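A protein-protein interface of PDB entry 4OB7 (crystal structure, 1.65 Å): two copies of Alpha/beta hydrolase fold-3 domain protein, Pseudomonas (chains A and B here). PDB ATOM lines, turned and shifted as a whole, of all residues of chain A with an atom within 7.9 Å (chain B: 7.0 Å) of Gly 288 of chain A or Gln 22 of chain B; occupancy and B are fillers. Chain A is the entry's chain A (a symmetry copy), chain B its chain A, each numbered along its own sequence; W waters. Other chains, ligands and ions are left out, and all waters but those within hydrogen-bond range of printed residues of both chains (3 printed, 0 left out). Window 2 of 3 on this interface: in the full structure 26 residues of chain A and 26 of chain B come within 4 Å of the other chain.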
ATOM      1  N   SER A 254      11.929  -1.628  21.096  1.00  0.00           N
ATOM      2  CA  SER A 254      11.798  -0.782  19.913  1.00  0.00           C
ATOM      3  C   SER A 254      11.699  -1.621  18.655  1.00  0.00           C
ATOM      4  O   SER A 254      10.890  -1.340  17.777  1.00  0.00           O
ATOM      5  CB  SER A 254      12.962   0.207  19.788  1.00  0.00           C
ATOM      6  OG  SER A 254      12.822   1.280  20.695  1.00  0.00           O
ATOM      7  N   LEU A 257       8.254  -2.956  18.176  1.00  0.00           N
ATOM      8  CA  LEU A 257       7.242  -1.952  17.826  1.00  0.00           C
ATOM      9  C   LEU A 257       7.434  -1.343  16.435  1.00  0.00           C
ATOM     10  O   LEU A 257       6.524  -0.730  15.887  1.00  0.00           O
ATOM     11  CB  LEU A 257       7.219  -0.840  18.874  1.00  0.00           C
ATOM     12  CG  LEU A 257       6.901  -1.280  20.300  1.00  0.00           C
ATOM     13  CD1 LEU A 257       7.110  -0.121  21.263  1.00  0.00           C
ATOM     14  CD2 LEU A 257       5.473  -1.793  20.381  1.00  0.00           C
ATOM     15  N   LYS A 258       8.623  -1.513  15.864  1.00  0.00           N
ATOM     16  CA  LYS A 258       8.935  -0.897  14.581  1.00  0.00           C
ATOM     17  C   LYS A 258       7.950  -1.314  13.487  1.00  0.00           C
ATOM     18  O   LYS A 258       7.613  -2.489  13.358  1.00  0.00           O
ATOM     19  CB  LYS A 258      10.374  -1.242  14.180  1.00  0.00           C
ATOM     20  CG  LYS A 258      10.796  -0.747  12.812  1.00  0.00           C
ATOM     21  CD  LYS A 258      12.274  -1.039  12.586  1.00  0.00           C
ATOM     22  CE  LYS A 258      12.678  -0.835  11.136  1.00  0.00           C
ATOM     23  NZ  LYS A 258      14.087  -1.268  10.902  1.00  0.00           N
ATOM     24  N   GLY A 259       7.459  -0.340  12.726  1.00  0.00           N
ATOM     25  CA  GLY A 259       6.592  -0.628  11.598  1.00  0.00           C
ATOM     26  C   GLY A 259       5.105  -0.668  11.910  1.00  0.00           C
ATOM     27  O   GLY A 259       4.290  -0.922  11.019  1.00  0.00           O
ATOM     28  N   LEU A 260       4.745  -0.417  13.166  1.00  0.00           N
ATOM     29  CA  LEU A 260       3.332  -0.379  13.540  1.00  0.00           C
ATOM     30  C   LEU A 260       2.652   0.826  12.897  1.00  0.00           C
ATOM     31  O   LEU A 260       3.319   1.794  12.514  1.00  0.00           O
ATOM     32  CB  LEU A 260       3.176  -0.352  15.065  1.00  0.00           C
ATOM     33  CG  LEU A 260       3.483  -1.673  15.764  1.00  0.00           C
ATOM     34  CD1 LEU A 260       3.479  -1.491  17.272  1.00  0.00           C
ATOM     35  CD2 LEU A 260       2.482  -2.743  15.377  1.00  0.00           C
ATOM     36  N   ARG A 282       5.243   7.013  23.957  1.00  0.00           N
ATOM     37  CA  ARG A 282       6.669   7.326  23.853  1.00  0.00           C
ATOM     38  C   ARG A 282       7.464   6.169  23.255  1.00  0.00           C
ATOM     39  O   ARG A 282       8.383   6.389  22.474  1.00  0.00           O
ATOM     40  CB  ARG A 282       7.267   7.694  25.213  1.00  0.00           C
ATOM     41  CG  ARG A 282       6.865   9.064  25.739  1.00  0.00           C
ATOM     42  CD  ARG A 282       7.744   9.427  26.922  1.00  0.00           C
ATOM     43  NE  ARG A 282       7.511  10.791  27.399  1.00  0.00           N
ATOM     44  CZ  ARG A 282       8.186  11.349  28.402  1.00  0.00           C
ATOM     45  NH1 ARG A 282       9.124  10.658  29.032  1.00  0.00           N
ATOM     46  NH2 ARG A 282       7.923  12.595  28.777  1.00  0.00           N
ATOM     47  N   LYS A 283       7.121   4.940  23.626  1.00  0.00           N
ATOM     48  CA  LYS A 283       7.815   3.787  23.059  1.00  0.00           C
ATOM     49  C   LYS A 283       7.561   3.653  21.562  1.00  0.00           C
ATOM     50  O   LYS A 283       8.467   3.321  20.805  1.00  0.00           O
ATOM     51  CB  LYS A 283       7.434   2.494  23.779  1.00  0.00           C
ATOM     52  CG  LYS A 283       8.172   2.299  25.092  1.00  0.00           C
ATOM     53  CD  LYS A 283       8.203   0.826  25.465  1.00  0.00           C
ATOM     54  CE  LYS A 283       9.577   0.385  25.953  1.00  0.00           C
ATOM     55  NZ  LYS A 283       9.556  -1.025  26.460  1.00  0.00           N
ATOM     56  N   LEU A 284       6.329   3.910  21.134  1.00  0.00           N
ATOM     57  CA  LEU A 284       6.036   3.890  19.706  1.00  0.00           C
ATOM     58  C   LEU A 284       6.868   4.943  18.982  1.00  0.00           C
ATOM     59  O   LEU A 284       7.495   4.662  17.958  1.00  0.00           O
ATOM     60  CB  LEU A 284       4.553   4.122  19.459  1.00  0.00           C
ATOM     61  CG  LEU A 284       3.594   3.045  19.950  1.00  0.00           C
ATOM     62  CD1 LEU A 284       2.177   3.550  19.760  1.00  0.00           C
ATOM     63  CD2 LEU A 284       3.795   1.743  19.175  1.00  0.00           C
ATOM     64  N   ASN A 285       6.888   6.156  19.531  1.00  0.00           N
ATOM     65  CA  ASN A 285       7.663   7.239  18.942  1.00  0.00           C
ATOM     66  C   ASN A 285       9.154   6.896  18.855  1.00  0.00           C
ATOM     67  O   ASN A 285       9.799   7.158  17.831  1.00  0.00           O
ATOM     68  CB  ASN A 285       7.420   8.544  19.715  1.00  0.00           C
ATOM     69  CG  ASN A 285       8.253   9.704  19.199  1.00  0.00           C
ATOM     70  OD1 ASN A 285       8.004  10.237  18.111  1.00  0.00           O
ATOM     71  ND2 ASN A 285       9.237  10.122  19.995  1.00  0.00           N
ATOM     72  N   ALA A 286       9.690   6.288  19.912  1.00  0.00           N
ATOM     73  CA  ALA A 286      11.111   5.927  19.950  1.00  0.00           C
ATOM     74  C   ALA A 286      11.428   4.849  18.920  1.00  0.00           C
ATOM     75  O   ALA A 286      12.576   4.721  18.475  1.00  0.00           O
ATOM     76  CB  ALA A 286      11.510   5.458  21.346  1.00  0.00           C
ATOM     77  N   ALA A 287      10.408   4.080  18.541  1.00  0.00           N
ATOM     78  CA  ALA A 287      10.564   3.014  17.549  1.00  0.00           C
ATOM     79  C   ALA A 287      10.287   3.504  16.129  1.00  0.00           C
ATOM     80  O   ALA A 287      10.260   2.709  15.186  1.00  0.00           O
ATOM     81  CB  ALA A 287       9.659   1.838  17.887  1.00  0.00           C
ATOM     82  N   GLY A 288      10.076   4.808  15.978  1.00  0.00           N
ATOM     83  CA  GLY A 288       9.862   5.393  14.666  1.00  0.00           C
ATOM     84  C   GLY A 288       8.436   5.374  14.159  1.00  0.00           C
ATOM     85  O   GLY A 288       8.171   5.804  13.033  1.00  0.00           O
ATOM     86  N   VAL A 289       7.516   4.872  14.979  1.00  0.00           N
ATOM     87  CA  VAL A 289       6.094   4.880  14.650  1.00  0.00           C
ATOM     88  C   VAL A 289       5.556   6.300  14.774  1.00  0.00           C
ATOM     89  O   VAL A 289       5.931   7.028  15.690  1.00  0.00           O
ATOM     90  CB  VAL A 289       5.310   3.944  15.602  1.00  0.00           C
ATOM     91  CG1 VAL A 289       3.812   3.962  15.292  1.00  0.00           C
ATOM     92  CG2 VAL A 289       5.855   2.516  15.494  1.00  0.00           C
ATOM     93  N   THR A 290       4.700   6.701  13.835  1.00  0.00           N
ATOM     94  CA  THR A 290       4.057   8.008  13.906  1.00  0.00           C
ATOM     95  C   THR A 290       3.019   7.992  15.010  1.00  0.00           C
ATOM     96  O   THR A 290       2.129   7.142  15.007  1.00  0.00           O
ATOM     97  CB  THR A 290       3.350   8.323  12.597  1.00  0.00           C
ATOM     98  OG1 THR A 290       4.335   8.510  11.568  1.00  0.00           O
ATOM     99  CG2 THR A 290       2.506   9.580  12.732  1.00  0.00           C
ATOM    100  N   VAL A 291       3.128   8.925  15.952  1.00  0.00           N
ATOM    101  CA  VAL A 291       2.202   8.977  17.078  1.00  0.00           C
ATOM    102  C   VAL A 291       1.745  10.396  17.356  1.00  0.00           C
ATOM    103  O   VAL A 291       2.544  11.327  17.336  1.00  0.00           O
ATOM    104  CB  VAL A 291       2.863   8.448  18.377  1.00  0.00           C
ATOM    105  CG1 VAL A 291       1.868   8.466  19.542  1.00  0.00           C
ATOM    106  CG2 VAL A 291       3.377   7.058  18.180  1.00  0.00           C
ATOM    107  N   GLY B  19      11.164  11.325  24.820  1.00  0.00           N
ATOM    108  CA  GLY B  19       9.743  11.534  24.615  1.00  0.00           C
ATOM    109  C   GLY B  19       9.401  12.648  23.644  1.00  0.00           C
ATOM    110  O   GLY B  19       8.240  12.787  23.261  1.00  0.00           O
ATOM    111  N   VAL B  20      10.386  13.446  23.239  1.00  0.00           N
ATOM    112  CA  VAL B  20      10.113  14.468  22.231  1.00  0.00           C
ATOM    113  C   VAL B  20       9.774  13.758  20.925  1.00  0.00           C
ATOM    114  O   VAL B  20      10.429  12.774  20.564  1.00  0.00           O
ATOM    115  CB  VAL B  20      11.301  15.445  22.047  1.00  0.00           C
ATOM    116  CG1 VAL B  20      11.064  16.380  20.843  1.00  0.00           C
ATOM    117  CG2 VAL B  20      11.509  16.258  23.316  1.00  0.00           C
ATOM    118  N   GLU B  21       8.733  14.228  20.238  1.00  0.00           N
ATOM    119  CA  GLU B  21       8.301  13.608  18.994  1.00  0.00           C
ATOM    120  C   GLU B  21       9.479  13.581  18.008  1.00  0.00           C
ATOM    121  O   GLU B  21      10.293  14.508  17.982  1.00  0.00           O
ATOM    122  CB  GLU B  21       7.086  14.356  18.432  1.00  0.00           C
ATOM    123  CG  GLU B  21       6.560  13.816  17.100  1.00  0.00           C
ATOM    124  CD  GLU B  21       7.329  14.363  15.914  1.00  0.00           C
ATOM    125  OE1 GLU B  21       7.794  15.519  15.994  1.00  0.00           O
ATOM    126  OE2 GLU B  21       7.472  13.633  14.905  1.00  0.00           O
ATOM    127  N   GLN B  22       9.567  12.519  17.208  1.00  0.00           N
ATOM    128  CA  GLN B  22      10.791  12.247  16.449  1.00  0.00           C
ATOM    129  C   GLN B  22      11.251  13.360  15.507  1.00  0.00           C
ATOM    130  O   GLN B  22      12.443  13.687  15.483  1.00  0.00           O
ATOM    131  CB  GLN B  22      10.709  10.903  15.719  1.00  0.00           C
ATOM    132  CG  GLN B  22       9.583  10.769  14.702  1.00  0.00           C
ATOM    133  CD  GLN B  22       9.606   9.403  14.035  1.00  0.00           C
ATOM    134  OE1 GLN B  22      10.577   8.652  14.173  1.00  0.00           O
ATOM    135  NE2 GLN B  22       8.544   9.075  13.309  1.00  0.00           N
ATOM    136  N   HIS B  23      10.332  13.934  14.735  1.00  0.00           N
ATOM    137  CA  HIS B  23      10.714  15.008  13.812  1.00  0.00           C
ATOM    138  C   HIS B  23      11.097  16.273  14.568  1.00  0.00           C
ATOM    139  O   HIS B  23      12.035  16.970  14.193  1.00  0.00           O
ATOM    140  CB  HIS B  23       9.606  15.279  12.785  1.00  0.00           C
ATOM    141  CG  HIS B  23       9.328  14.105  11.904  1.00  0.00           C
ATOM    142  ND1 HIS B  23      10.184  13.715  10.896  1.00  0.00           N
ATOM    143  CD2 HIS B  23       8.312  13.207  11.903  1.00  0.00           C
ATOM    144  CE1 HIS B  23       9.700  12.638  10.302  1.00  0.00           C
ATOM    145  NE2 HIS B  23       8.566  12.311  10.895  1.00  0.00           N
ATOM    146  N   THR B  24      10.371  16.558  15.642  1.00  0.00           N
ATOM    147  CA  THR B  24      10.683  17.698  16.501  1.00  0.00           C
ATOM    148  C   THR B  24      12.079  17.563  17.126  1.00  0.00           C
ATOM    149  O   THR B  24      12.845  18.529  17.197  1.00  0.00           O
ATOM    150  CB  THR B  24       9.627  17.821  17.606  1.00  0.00           C
ATOM    151  OG1 THR B  24       8.345  18.018  16.993  1.00  0.00           O
ATOM    152  CG2 THR B  24       9.931  19.003  18.524  1.00  0.00           C
ATOM    153  N   GLN B  25      12.407  16.357  17.569  1.00  0.00           N
ATOM    154  CA  GLN B  25      13.732  16.101  18.125  1.00  0.00           C
ATOM    155  C   GLN B  25      14.825  16.340  17.080  1.00  0.00           C
ATOM    156  O   GLN B  25      15.856  16.954  17.381  1.00  0.00           O
ATOM    157  CB  GLN B  25      13.814  14.674  18.681  1.00  0.00           C
ATOM    158  CG  GLN B  25      15.184  14.321  19.265  1.00  0.00           C
ATOM    159  CD  GLN B  25      15.562  15.166  20.477  1.00  0.00           C
ATOM    160  OE1 GLN B  25      14.708  15.569  21.271  1.00  0.00           O
ATOM    161  NE2 GLN B  25      16.857  15.440  20.620  1.00  0.00           N
ATOM    162  N   ALA B  26      14.595  15.871  15.856  1.00  0.00           N
ATOM    163  CA  ALA B  26      15.553  16.082  14.772  1.00  0.00           C
ATOM    164  C   ALA B  26      15.718  17.574  14.486  1.00  0.00           C
ATOM    165  O   ALA B  26      16.821  18.048  14.218  1.00  0.00           O
ATOM    166  CB  ALA B  26      15.117  15.339  13.523  1.00  0.00           C
ATOM    167  N   PHE B  27      14.613  18.307  14.554  1.00  0.00           N
ATOM    168  CA  PHE B  27      14.626  19.756  14.373  1.00  0.00           C
ATOM    169  C   PHE B  27      15.476  20.445  15.440  1.00  0.00           C
ATOM    170  O   PHE B  27      16.272  21.334  15.130  1.00  0.00           O
ATOM    171  CB  PHE B  27      13.175  20.267  14.389  1.00  0.00           C
ATOM    172  CG  PHE B  27      13.034  21.756  14.540  1.00  0.00           C
ATOM    173  CD1 PHE B  27      13.261  22.601  13.465  1.00  0.00           C
ATOM    174  CD2 PHE B  27      12.621  22.307  15.745  1.00  0.00           C
ATOM    175  CE1 PHE B  27      13.107  23.970  13.599  1.00  0.00           C
ATOM    176  CE2 PHE B  27      12.471  23.680  15.889  1.00  0.00           C
ATOM    177  CZ  PHE B  27      12.712  24.512  14.808  1.00  0.00           C
ATOM    178  N   GLU B  29      17.880  19.131  17.192  1.00  0.00           N
ATOM    179  CA  GLU B  29      19.274  18.753  16.970  1.00  0.00           C
ATOM    180  C   GLU B  29      19.901  19.541  15.825  1.00  0.00           C
ATOM    181  O   GLU B  29      21.072  19.917  15.890  1.00  0.00           O
ATOM    182  CB  GLU B  29      19.386  17.238  16.747  1.00  0.00           C
ATOM    183  CG  GLU B  29      19.113  16.443  18.015  1.00  0.00           C
ATOM    184  CD  GLU B  29      18.934  14.956  17.770  1.00  0.00           C
ATOM    185  OE1 GLU B  29      18.924  14.536  16.594  1.00  0.00           O
ATOM    186  OE2 GLU B  29      18.787  14.209  18.757  1.00  0.00           O
ATOM    187  N   GLY B 298       4.976  15.243  23.399  1.00  0.00           N
ATOM    188  CA  GLY B 298       6.033  15.222  22.400  1.00  0.00           C
ATOM    189  C   GLY B 298       6.333  16.560  21.740  1.00  0.00           C
ATOM    190  O   GLY B 298       7.318  16.679  21.006  1.00  0.00           O
ATOM    191  N   MET B 299       5.494  17.565  21.990  1.00  0.00           N
ATOM    192  CA  MET B 299       5.603  18.842  21.290  1.00  0.00           C
ATOM    193  C   MET B 299       6.424  19.861  22.055  1.00  0.00           C
ATOM    194  O   MET B 299       6.463  19.841  23.280  1.00  0.00           O
ATOM    195  CB  MET B 299       4.209  19.443  21.041  1.00  0.00           C
ATOM    196  CG  MET B 299       3.273  18.595  20.177  1.00  0.00           C
ATOM    197  SD  MET B 299       3.780  18.408  18.451  1.00  0.00           S
ATOM    198  CE  MET B 299       4.675  16.866  18.523  1.00  0.00           C
ATOM    199  N   VAL B 312       4.542  17.784  10.696  1.00  0.00           N
ATOM    200  CA  VAL B 312       4.615  16.765  11.737  1.00  0.00           C
ATOM    201  C   VAL B 312       3.190  16.285  12.001  1.00  0.00           C
ATOM    202  O   VAL B 312       2.287  17.102  12.189  1.00  0.00           O
ATOM    203  CB  VAL B 312       5.229  17.339  13.021  1.00  0.00           C
ATOM    204  CG1 VAL B 312       5.090  16.347  14.164  1.00  0.00           C
ATOM    205  CG2 VAL B 312       6.700  17.696  12.790  1.00  0.00           C
ATOM    206  N   PRO B 313       2.965  14.967  11.975  1.00  0.00           N
ATOM    207  CA  PRO B 313       1.577  14.495  12.075  1.00  0.00           C
ATOM    208  C   PRO B 313       0.830  14.988  13.317  1.00  0.00           C
ATOM    209  O   PRO B 313      -0.330  15.358  13.185  1.00  0.00           O
ATOM    210  CB  PRO B 313       1.726  12.971  12.068  1.00  0.00           C
ATOM    211  CG  PRO B 313       2.974  12.754  11.222  1.00  0.00           C
ATOM    212  CD  PRO B 313       3.899  13.877  11.633  1.00  0.00           C
HETATM  213  O   HOH W   1       6.289  12.374  25.307  1.00  0.00           O
HETATM  214  O   HOH W   2       6.228  10.541  12.072  1.00  0.00           O
HETATM  215  O   HOH W   3      12.333   7.869  16.735  1.00  0.00           O
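The backbone NH (N) of His 23 of chain B is in hydrogen-bond range of the side-chain carboxylate (OE2) of Glu 21 of chain B, 2.9 Å away. The side-chain carboxylate of Glu 21 of chain B sits at hydrogen-bond distance from the side-chain hydroxyl of Thr 24 of chain B (2.7 Å). O of Gly 298 of chain B lies within hydrogen-bond range of N of Glu 21 of chain B.
ND2 of Asn 285 of chain A is in hydrogen-bond range of O of Val 20 of chain B (3.0 Å). OD1 of Asn 285 of chain A lies within hydrogen-bond range of N of Gln 22 of chain B. The side-chain amide nitrogen of Gln 22 of chain B sits at hydrogen-bond distance from the backbone carbonyl oxygen of Gly 288 of chain A (3.3 Å).
Ser 254 of chain A touches none of the printed residues of chain B. Of the printed residues of chain B, Asn 285 of chain A touches Val 20, Glu 21 and Gln 22. Gly 288 of chain A touches just one residue of chain B: Gln 22 (3.3 Å). Of the printed residues of chain A, Gly 19 of chain B touches Arg 282. Of the printed residues of chain A, Val 20 of chain B touches Asn 285. Of chain A, only Asn 285 comes within 4 Å of Glu 21 of chain B. Gln 22 of chain B touches two residues of chain A. Gly 298 of chain B touches none of the printed residues of chain A. Of the printed residues of chain A, Pro 313 of chain B touches Thr 290 (3.5 Å). The nearest residue of chain B that does not touch Gly 288 of chain A is His 23 of chain B (6.9 Å). The nearest printed residue of chain A that does not touch Gly 19 of chain B is Asn 285 of chain A (4.3 Å).
Of the 15 printed residues of chain A, 4 touch a printed residue of chain B. Among the printed residues, no Asp or Glu carboxylate lies within 4 Å of a Lys or Arg side-chain nitrogen of the other chain.
Water W2 lies within hydrogen-bond range of the side-chain hydroxyl of Thr 290 of chain A (2.8 Å), the side-chain amide nitrogen of Gln 22 of chain B (3.0 Å) and a ring nitrogen (NE2) of His 23 of chain B (3.2 Å). Water W3 lies within hydrogen-bond range of the backbone carbonyl oxygen of Asn 285 of chain A and the side-chain amide oxygen of Gln 22 of chain B. Water W1 lies within hydrogen-bond range of the backbone carbonyl oxygen (O) of Gly 19 of chain B (2.9 Å) and the guanidinium group (NE) of Arg 282 of chain A (2.9 Å).
No position is printed for both chains.
Among the printed residues, pairs that only touch across the chains: Arg 282 of chain A with Gly 19 of chain B (3.6 Å), Asn 285 of chain A with Glu 21 of chain B (3.5 Å) and Thr 290 of chain A with Pro 313 of chain B (3.5 Å).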
